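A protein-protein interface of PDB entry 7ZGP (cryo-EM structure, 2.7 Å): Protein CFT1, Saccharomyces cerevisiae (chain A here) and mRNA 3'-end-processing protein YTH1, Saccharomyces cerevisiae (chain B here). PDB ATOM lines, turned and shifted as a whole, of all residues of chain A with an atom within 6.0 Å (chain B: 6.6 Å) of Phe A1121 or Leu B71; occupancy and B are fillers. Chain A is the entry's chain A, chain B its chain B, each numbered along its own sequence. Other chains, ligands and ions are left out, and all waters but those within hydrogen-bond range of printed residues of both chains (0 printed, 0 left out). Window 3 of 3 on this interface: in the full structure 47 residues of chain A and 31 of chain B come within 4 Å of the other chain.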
ATOM      1  N   LYS A1104     -13.408   1.024   4.647  1.00  0.00           N
ATOM      2  CA  LYS A1104     -12.648   2.204   5.028  1.00  0.00           C
ATOM      3  C   LYS A1104     -12.126   2.019   6.445  1.00  0.00           C
ATOM      4  O   LYS A1104     -12.820   1.457   7.295  1.00  0.00           O
ATOM      5  CB  LYS A1104     -13.521   3.461   4.949  1.00  0.00           C
ATOM      6  CG  LYS A1104     -12.776   4.759   5.154  1.00  0.00           C
ATOM      7  CD  LYS A1104     -12.053   5.158   3.891  1.00  0.00           C
ATOM      8  CE  LYS A1104     -13.038   5.432   2.770  1.00  0.00           C
ATOM      9  NZ  LYS A1104     -13.868   6.632   3.058  1.00  0.00           N
ATOM     10  N   VAL A1105     -10.906   2.490   6.691  1.00  0.00           N
ATOM     11  CA  VAL A1105     -10.359   2.584   8.040  1.00  0.00           C
ATOM     12  C   VAL A1105      -9.897   4.016   8.263  1.00  0.00           C
ATOM     13  O   VAL A1105      -9.181   4.582   7.429  1.00  0.00           O
ATOM     14  CB  VAL A1105      -9.207   1.588   8.280  1.00  0.00           C
ATOM     15  CG1 VAL A1105      -9.754   0.183   8.456  1.00  0.00           C
ATOM     16  CG2 VAL A1105      -8.212   1.624   7.139  1.00  0.00           C
ATOM     17  N   LEU A1106     -10.320   4.606   9.378  1.00  0.00           N
ATOM     18  CA  LEU A1106      -9.985   5.979   9.723  1.00  0.00           C
ATOM     19  C   LEU A1106      -9.197   5.989  11.023  1.00  0.00           C
ATOM     20  O   LEU A1106      -9.610   5.369  12.006  1.00  0.00           O
ATOM     21  CB  LEU A1106     -11.245   6.836   9.866  1.00  0.00           C
ATOM     22  CG  LEU A1106     -11.863   7.410   8.591  1.00  0.00           C
ATOM     23  CD1 LEU A1106     -12.907   8.456   8.937  1.00  0.00           C
ATOM     24  CD2 LEU A1106     -10.796   7.997   7.690  1.00  0.00           C
ATOM     25  N   VAL A1107      -8.071   6.694  11.025  1.00  0.00           N
ATOM     26  CA  VAL A1107      -7.259   6.885  12.220  1.00  0.00           C
ATOM     27  C   VAL A1107      -7.568   8.259  12.790  1.00  0.00           C
ATOM     28  O   VAL A1107      -7.495   9.267  12.077  1.00  0.00           O
ATOM     29  CB  VAL A1107      -5.759   6.744  11.912  1.00  0.00           C
ATOM     30  CG1 VAL A1107      -4.937   6.918  13.179  1.00  0.00           C
ATOM     31  CG2 VAL A1107      -5.476   5.403  11.270  1.00  0.00           C
ATOM     32  N   VAL A1119      -7.088  11.708  11.148  1.00  0.00           N
ATOM     33  CA  VAL A1119      -5.794  12.207  10.698  1.00  0.00           C
ATOM     34  C   VAL A1119      -5.277  11.375   9.531  1.00  0.00           C
ATOM     35  O   VAL A1119      -4.484  11.858   8.717  1.00  0.00           O
ATOM     36  CB  VAL A1119      -4.774  12.224  11.852  1.00  0.00           C
ATOM     37  CG1 VAL A1119      -5.109  13.333  12.836  1.00  0.00           C
ATOM     38  CG2 VAL A1119      -4.737  10.877  12.550  1.00  0.00           C
ATOM     39  N   ALA A1120      -5.726  10.127   9.431  1.00  0.00           N
ATOM     40  CA  ALA A1120      -5.270   9.224   8.385  1.00  0.00           C
ATOM     41  C   ALA A1120      -6.475   8.549   7.739  1.00  0.00           C
ATOM     42  O   ALA A1120      -7.615   8.702   8.184  1.00  0.00           O
ATOM     43  CB  ALA A1120      -4.285   8.185   8.935  1.00  0.00           C
ATOM     44  N   PHE A1121      -6.206   7.786   6.680  1.00  0.00           N
ATOM     45  CA  PHE A1121      -7.252   7.238   5.828  1.00  0.00           C
ATOM     46  C   PHE A1121      -6.676   6.140   4.940  1.00  0.00           C
ATOM     47  O   PHE A1121      -5.622   6.321   4.323  1.00  0.00           O
ATOM     48  CB  PHE A1121      -7.880   8.373   5.003  1.00  0.00           C
ATOM     49  CG  PHE A1121      -8.265   7.993   3.596  1.00  0.00           C
ATOM     50  CD1 PHE A1121      -9.169   6.975   3.342  1.00  0.00           C
ATOM     51  CD2 PHE A1121      -7.773   8.718   2.525  1.00  0.00           C
ATOM     52  CE1 PHE A1121      -9.521   6.651   2.047  1.00  0.00           C
ATOM     53  CE2 PHE A1121      -8.123   8.400   1.232  1.00  0.00           C
ATOM     54  CZ  PHE A1121      -9.000   7.367   0.993  1.00  0.00           C
ATOM     55  N   LEU A1122      -7.359   4.999   4.872  1.00  0.00           N
ATOM     56  CA  LEU A1122      -6.957   3.915   3.990  1.00  0.00           C
ATOM     57  C   LEU A1122      -8.198   3.139   3.578  1.00  0.00           C
ATOM     58  O   LEU A1122      -9.130   2.986   4.370  1.00  0.00           O
ATOM     59  CB  LEU A1122      -5.935   2.994   4.667  1.00  0.00           C
ATOM     60  CG  LEU A1122      -5.350   1.863   3.821  1.00  0.00           C
ATOM     61  CD1 LEU A1122      -3.842   1.969   3.759  1.00  0.00           C
ATOM     62  CD2 LEU A1122      -5.764   0.516   4.385  1.00  0.00           C
ATOM     63  N   ASP A1123      -8.208   2.662   2.338  1.00  0.00           N
ATOM     64  CA  ASP A1123      -9.348   1.952   1.776  1.00  0.00           C
ATOM     65  C   ASP A1123      -9.233   0.458   2.043  1.00  0.00           C
ATOM     66  O   ASP A1123      -8.130  -0.096   2.080  1.00  0.00           O
ATOM     67  CB  ASP A1123      -9.461   2.211   0.274  1.00  0.00           C
ATOM     68  CG  ASP A1123     -10.213   3.488  -0.039  1.00  0.00           C
ATOM     69  OD1 ASP A1123     -11.343   3.651   0.467  1.00  0.00           O
ATOM     70  OD2 ASP A1123      -9.675   4.333  -0.785  1.00  0.00           O
ATOM     71  N   MET A1159      -0.715   6.263   5.862  1.00  0.00           N
ATOM     72  CA  MET A1159      -1.058   4.853   6.013  1.00  0.00           C
ATOM     73  C   MET A1159      -0.334   4.122   4.888  1.00  0.00           C
ATOM     74  O   MET A1159      -0.893   3.903   3.811  1.00  0.00           O
ATOM     75  CB  MET A1159      -2.561   4.632   5.966  1.00  0.00           C
ATOM     76  CG  MET A1159      -3.285   5.023   7.242  1.00  0.00           C
ATOM     77  SD  MET A1159      -3.152   3.753   8.512  1.00  0.00           S
ATOM     78  CE  MET A1159      -4.828   3.125   8.533  1.00  0.00           C
ATOM     79  N   VAL B  66      -6.021  19.497   0.175  1.00  0.00           N
ATOM     80  CA  VAL B  66      -6.122  18.053   0.010  1.00  0.00           C
ATOM     81  C   VAL B  66      -6.563  17.724  -1.408  1.00  0.00           C
ATOM     82  O   VAL B  66      -7.485  18.346  -1.951  1.00  0.00           O
ATOM     83  CB  VAL B  66      -7.092  17.469   1.047  1.00  0.00           C
ATOM     84  CG1 VAL B  66      -7.224  15.965   0.872  1.00  0.00           C
ATOM     85  CG2 VAL B  66      -6.623  17.806   2.450  1.00  0.00           C
ATOM     86  N   CYS B  67      -5.903  16.740  -2.014  1.00  0.00           N
ATOM     87  CA  CYS B  67      -6.245  16.321  -3.367  1.00  0.00           C
ATOM     88  C   CYS B  67      -7.602  15.632  -3.379  1.00  0.00           C
ATOM     89  O   CYS B  67      -7.808  14.637  -2.680  1.00  0.00           O
ATOM     90  CB  CYS B  67      -5.165  15.389  -3.912  1.00  0.00           C
ATOM     91  SG  CYS B  67      -5.518  14.702  -5.541  1.00  0.00           S
ATOM     92  N   ARG B  68      -8.527  16.163  -4.181  1.00  0.00           N
ATOM     93  CA  ARG B  68      -9.863  15.582  -4.249  1.00  0.00           C
ATOM     94  C   ARG B  68      -9.845  14.199  -4.888  1.00  0.00           C
ATOM     95  O   ARG B  68     -10.676  13.350  -4.543  1.00  0.00           O
ATOM     96  CB  ARG B  68     -10.805  16.518  -5.011  1.00  0.00           C
ATOM     97  CG  ARG B  68     -10.605  16.538  -6.519  1.00  0.00           C
ATOM     98  CD  ARG B  68     -11.650  17.400  -7.203  1.00  0.00           C
ATOM     99  NE  ARG B  68     -11.317  18.819  -7.138  1.00  0.00           N
ATOM    100  CZ  ARG B  68     -11.914  19.692  -6.339  1.00  0.00           C
ATOM    101  NH1 ARG B  68     -12.886  19.328  -5.520  1.00  0.00           N
ATOM    102  NH2 ARG B  68     -11.526  20.965  -6.364  1.00  0.00           N
ATOM    103  N   HIS B  69      -8.916  13.951  -5.812  1.00  0.00           N
ATOM    104  CA  HIS B  69      -8.822  12.639  -6.440  1.00  0.00           C
ATOM    105  C   HIS B  69      -8.162  11.616  -5.528  1.00  0.00           C
ATOM    106  O   HIS B  69      -8.464  10.422  -5.623  1.00  0.00           O
ATOM    107  CB  HIS B  69      -8.056  12.747  -7.758  1.00  0.00           C
ATOM    108  CG  HIS B  69      -8.547  13.844  -8.650  1.00  0.00           C
ATOM    109  ND1 HIS B  69      -8.025  15.119  -8.616  1.00  0.00           N
ATOM    110  CD2 HIS B  69      -9.519  13.860  -9.591  1.00  0.00           C
ATOM    111  CE1 HIS B  69      -8.652  15.871  -9.503  1.00  0.00           C
ATOM    112  NE2 HIS B  69      -9.563  15.132 -10.108  1.00  0.00           N
ATOM    113  N   TRP B  70      -7.262  12.060  -4.649  1.00  0.00           N
ATOM    114  CA  TRP B  70      -6.651  11.150  -3.688  1.00  0.00           C
ATOM    115  C   TRP B  70      -7.678  10.614  -2.698  1.00  0.00           C
ATOM    116  O   TRP B  70      -7.610   9.447  -2.298  1.00  0.00           O
ATOM    117  CB  TRP B  70      -5.512  11.856  -2.954  1.00  0.00           C
ATOM    118  CG  TRP B  70      -4.863  11.014  -1.905  1.00  0.00           C
ATOM    119  CD1 TRP B  70      -3.970  10.003  -2.102  1.00  0.00           C
ATOM    120  CD2 TRP B  70      -5.050  11.115  -0.490  1.00  0.00           C
ATOM    121  NE1 TRP B  70      -3.594   9.463  -0.898  1.00  0.00           N
ATOM    122  CE2 TRP B  70      -4.242  10.128   0.107  1.00  0.00           C
ATOM    123  CE3 TRP B  70      -5.823  11.940   0.329  1.00  0.00           C
ATOM    124  CZ2 TRP B  70      -4.187   9.946   1.485  1.00  0.00           C
ATOM    125  CZ3 TRP B  70      -5.767  11.758   1.695  1.00  0.00           C
ATOM    126  CH2 TRP B  70      -4.953  10.770   2.260  1.00  0.00           C
ATOM    127  N   LEU B  71      -8.632  11.454  -2.289  1.00  0.00           N
ATOM    128  CA  LEU B  71      -9.653  11.013  -1.345  1.00  0.00           C
ATOM    129  C   LEU B  71     -10.513   9.900  -1.924  1.00  0.00           C
ATOM    130  O   LEU B  71     -10.996   9.038  -1.182  1.00  0.00           O
ATOM    131  CB  LEU B  71     -10.527  12.195  -0.930  1.00  0.00           C
ATOM    132  CG  LEU B  71      -9.810  13.322  -0.188  1.00  0.00           C
ATOM    133  CD1 LEU B  71     -10.705  14.541  -0.087  1.00  0.00           C
ATOM    134  CD2 LEU B  71      -9.373  12.861   1.190  1.00  0.00           C
ATOM    135  N   ARG B  72     -10.717   9.900  -3.237  1.00  0.00           N
ATOM    136  CA  ARG B  72     -11.446   8.839  -3.914  1.00  0.00           C
ATOM    137  C   ARG B  72     -10.543   7.695  -4.350  1.00  0.00           C
ATOM    138  O   ARG B  72     -11.025   6.748  -4.977  1.00  0.00           O
ATOM    139  CB  ARG B  72     -12.184   9.401  -5.132  1.00  0.00           C
ATOM    140  CG  ARG B  72     -12.972  10.666  -4.849  1.00  0.00           C
ATOM    141  CD  ARG B  72     -14.130  10.397  -3.905  1.00  0.00           C
ATOM    142  NE  ARG B  72     -14.960   9.293  -4.370  1.00  0.00           N
ATOM    143  CZ  ARG B  72     -15.536   8.402  -3.575  1.00  0.00           C
ATOM    144  NH1 ARG B  72     -15.397   8.454  -2.261  1.00  0.00           N
ATOM    145  NH2 ARG B  72     -16.270   7.431  -4.113  1.00  0.00           N
ATOM    146  N   GLY B  73      -9.254   7.761  -4.034  1.00  0.00           N
ATOM    147  CA  GLY B  73      -8.308   6.761  -4.494  1.00  0.00           C
ATOM    148  C   GLY B  73      -8.108   6.771  -5.992  1.00  0.00           C
ATOM    149  O   GLY B  73      -7.910   5.709  -6.594  1.00  0.00           O
ATOM    150  N   LEU B  74      -8.151   7.949  -6.611  1.00  0.00           N
ATOM    151  CA  LEU B  74      -8.067   8.072  -8.061  1.00  0.00           C
ATOM    152  C   LEU B  74      -7.131   9.205  -8.452  1.00  0.00           C
ATOM    153  O   LEU B  74      -7.386   9.939  -9.413  1.00  0.00           O
ATOM    154  CB  LEU B  74      -9.451   8.287  -8.672  1.00  0.00           C
ATOM    155  CG  LEU B  74     -10.435   7.126  -8.550  1.00  0.00           C
ATOM    156  CD1 LEU B  74     -11.832   7.567  -8.944  1.00  0.00           C
ATOM    157  CD2 LEU B  74      -9.980   5.953  -9.396  1.00  0.00           C
ATOM    158  N   CYS B  75      -6.032   9.365  -7.720  1.00  0.00           N
ATOM    159  CA  CYS B  75      -5.038  10.384  -8.038  1.00  0.00           C
ATOM    160  C   CYS B  75      -4.025   9.800  -9.015  1.00  0.00           C
ATOM    161  O   CYS B  75      -3.329   8.833  -8.690  1.00  0.00           O
ATOM    162  CB  CYS B  75      -4.339  10.881  -6.775  1.00  0.00           C
ATOM    163  SG  CYS B  75      -3.107  12.169  -7.072  1.00  0.00           S
ATOM    164  N   LEU B  84      -2.364  18.195  -1.556  1.00  0.00           N
ATOM    165  CA  LEU B  84      -1.992  17.433  -0.373  1.00  0.00           C
ATOM    166  C   LEU B  84      -2.587  16.031  -0.419  1.00  0.00           C
ATOM    167  O   LEU B  84      -3.788  15.860  -0.644  1.00  0.00           O
ATOM    168  CB  LEU B  84      -2.454  18.163   0.885  1.00  0.00           C
ATOM    169  CG  LEU B  84      -2.135  17.480   2.212  1.00  0.00           C
ATOM    170  CD1 LEU B  84      -0.640  17.275   2.344  1.00  0.00           C
ATOM    171  CD2 LEU B  84      -2.673  18.290   3.373  1.00  0.00           C
ATOM    172  N   GLU B  86      -2.635  14.100   2.211  1.00  0.00           N
ATOM    173  CA  GLU B  86      -2.772  13.780   3.652  1.00  0.00           C
ATOM    174  C   GLU B  86      -4.208  14.083   4.072  1.00  0.00           C
ATOM    175  O   GLU B  86      -4.750  15.105   3.617  1.00  0.00           O
ATOM    176  CB  GLU B  86      -1.781  14.600   4.478  1.00  0.00           C
ATOM    177  CG  GLU B  86      -1.853  14.320   5.968  1.00  0.00           C
ATOM    178  CD  GLU B  86      -0.869  15.124   6.798  1.00  0.00           C
ATOM    179  OE1 GLU B  86      -0.125  15.931   6.208  1.00  0.00           O
ATOM    180  OE2 GLU B  86      -0.849  14.942   8.031  1.00  0.00           O
ATOM    181  N   TYR B  87      -4.794  13.223   4.899  1.00  0.00           N
ATOM    182  CA  TYR B  87      -6.167  13.407   5.370  1.00  0.00           C
ATOM    183  C   TYR B  87      -6.195  14.509   6.430  1.00  0.00           C
ATOM    184  O   TYR B  87      -6.433  14.283   7.618  1.00  0.00           O
ATOM    185  CB  TYR B  87      -6.730  12.099   5.905  1.00  0.00           C
ATOM    186  CG  TYR B  87      -8.239  12.042   5.884  1.00  0.00           C
ATOM    187  CD1 TYR B  87      -8.947  12.348   4.733  1.00  0.00           C
ATOM    188  CD2 TYR B  87      -8.954  11.685   7.016  1.00  0.00           C
ATOM    189  CE1 TYR B  87     -10.326  12.299   4.709  1.00  0.00           C
ATOM    190  CE2 TYR B  87     -10.333  11.633   7.002  1.00  0.00           C
ATOM    191  CZ  TYR B  87     -11.014  11.941   5.846  1.00  0.00           C
ATOM    192  OH  TYR B  87     -12.388  11.890   5.829  1.00  0.00           O
ATOM    193  N   ASN B  88      -5.940  15.729   5.970  1.00  0.00           N
ATOM    194  CA  ASN B  88      -5.982  16.914   6.814  1.00  0.00           C
ATOM    195  C   ASN B  88      -7.331  17.593   6.614  1.00  0.00           C
ATOM    196  O   ASN B  88      -7.638  18.059   5.512  1.00  0.00           O
ATOM    197  CB  ASN B  88      -4.835  17.865   6.476  1.00  0.00           C
ATOM    198  CG  ASN B  88      -4.478  18.777   7.629  1.00  0.00           C
ATOM    199  OD1 ASN B  88      -5.347  19.203   8.388  1.00  0.00           O
ATOM    200  ND2 ASN B  88      -3.193  19.078   7.772  1.00  0.00           N
ATOM    201  N   MET B  92      -8.928  20.671   3.588  1.00  0.00           N
ATOM    202  CA  MET B  92      -9.777  20.218   2.501  1.00  0.00           C
ATOM    203  C   MET B  92     -10.376  21.412   1.758  1.00  0.00           C
ATOM    204  O   MET B  92     -10.600  22.473   2.346  1.00  0.00           O
ATOM    205  CB  MET B  92     -10.900  19.329   3.030  1.00  0.00           C
ATOM    206  CG  MET B  92     -10.441  18.229   3.965  1.00  0.00           C
ATOM    207  SD  MET B  92     -10.464  16.611   3.177  1.00  0.00           S
ATOM    208  CE  MET B  92     -12.161  16.547   2.608  1.00  0.00           C
ATOM    209  N   PRO B  93     -10.643  21.264   0.459  1.00  0.00           N
ATOM    210  CA  PRO B  93     -11.338  22.334  -0.288  1.00  0.00           C
ATOM    211  C   PRO B  93     -12.845  22.285  -0.067  1.00  0.00           C
ATOM    212  O   PRO B  93     -13.636  21.957  -0.959  1.00  0.00           O
ATOM    213  CB  PRO B  93     -10.934  22.036  -1.735  1.00  0.00           C
ATOM    214  CG  PRO B  93     -10.771  20.553  -1.771  1.00  0.00           C
ATOM    215  CD  PRO B  93     -10.275  20.131  -0.409  1.00  0.00           C
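O of Val A1119 sits close to O of Tyr B87 (3.3 Å).
The side-chain sulfur (SG) of Cys B67 sits close to the backbone NH (N) of Trp B70. The backbone NH of Ala A1120 sits at hydrogen-bond distance from the backbone carbonyl oxygen of Val A1107, at 3.3 Å. The backbone NH of Val A1119 is in hydrogen-bond range of the backbone carbonyl oxygen of Val A1107 (2.6 Å).
Leu A1106 touches Tyr B87. Tyr B87 touches Ala A1120 (CD2 to O, 3.5 Å). Phe A1121 touches Trp B70. Phe A1121 touches Leu B71. CG of Tyr B87 touches CB of Phe A1121, at 3.8 Å.
Of chain B, only Trp B70 (3.5 Å), Leu B71 (3.4 Å) and Tyr B87 (3.8 Å) come within 4 Å of Phe A1121. Of chain A, only Phe A1121 (3.4 Å) comes within 4 Å of Leu B71. Of the printed residues of chain B, Ala A1120 touches Tyr B87 (3.5 Å). Printed residues of chain A within 4 Å of Tyr B87: Leu A1106 (3.7 Å), Val A1119 (3.3 Å), Ala A1120 (3.5 Å) and Phe A1121 (3.8 Å). Printed residues of chain A within 4 Å of Trp B70: Phe A1121. Printed residues of chain B within 4 Å of Val A1119: Tyr B87 (3.3 Å). Val A1107 touches none of the printed residues of chain B. The nearest residue of chain B that does not touch Phe A1121 is Gly B73 (5.0 Å). The nearest residue of chain A that does not touch Leu B71 is Asp A1123 (4.9 Å).
Of the 16 printed residues of chain B, 3 touch a printed residue of chain A. Printed residues of chain A that touch a printed residue of chain B: Leu A1106, Val A1119, Ala A1120 and Phe A1121. Along chain A the printed residues that touch a printed residue of chain B span positions 1106 to 1121. Among the printed residues, 6 pairs touch across the chains. Among the printed residues, no Asp or Glu carboxylate lies within 4 Å of a Lys or Arg side-chain nitrogen of the other chain.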
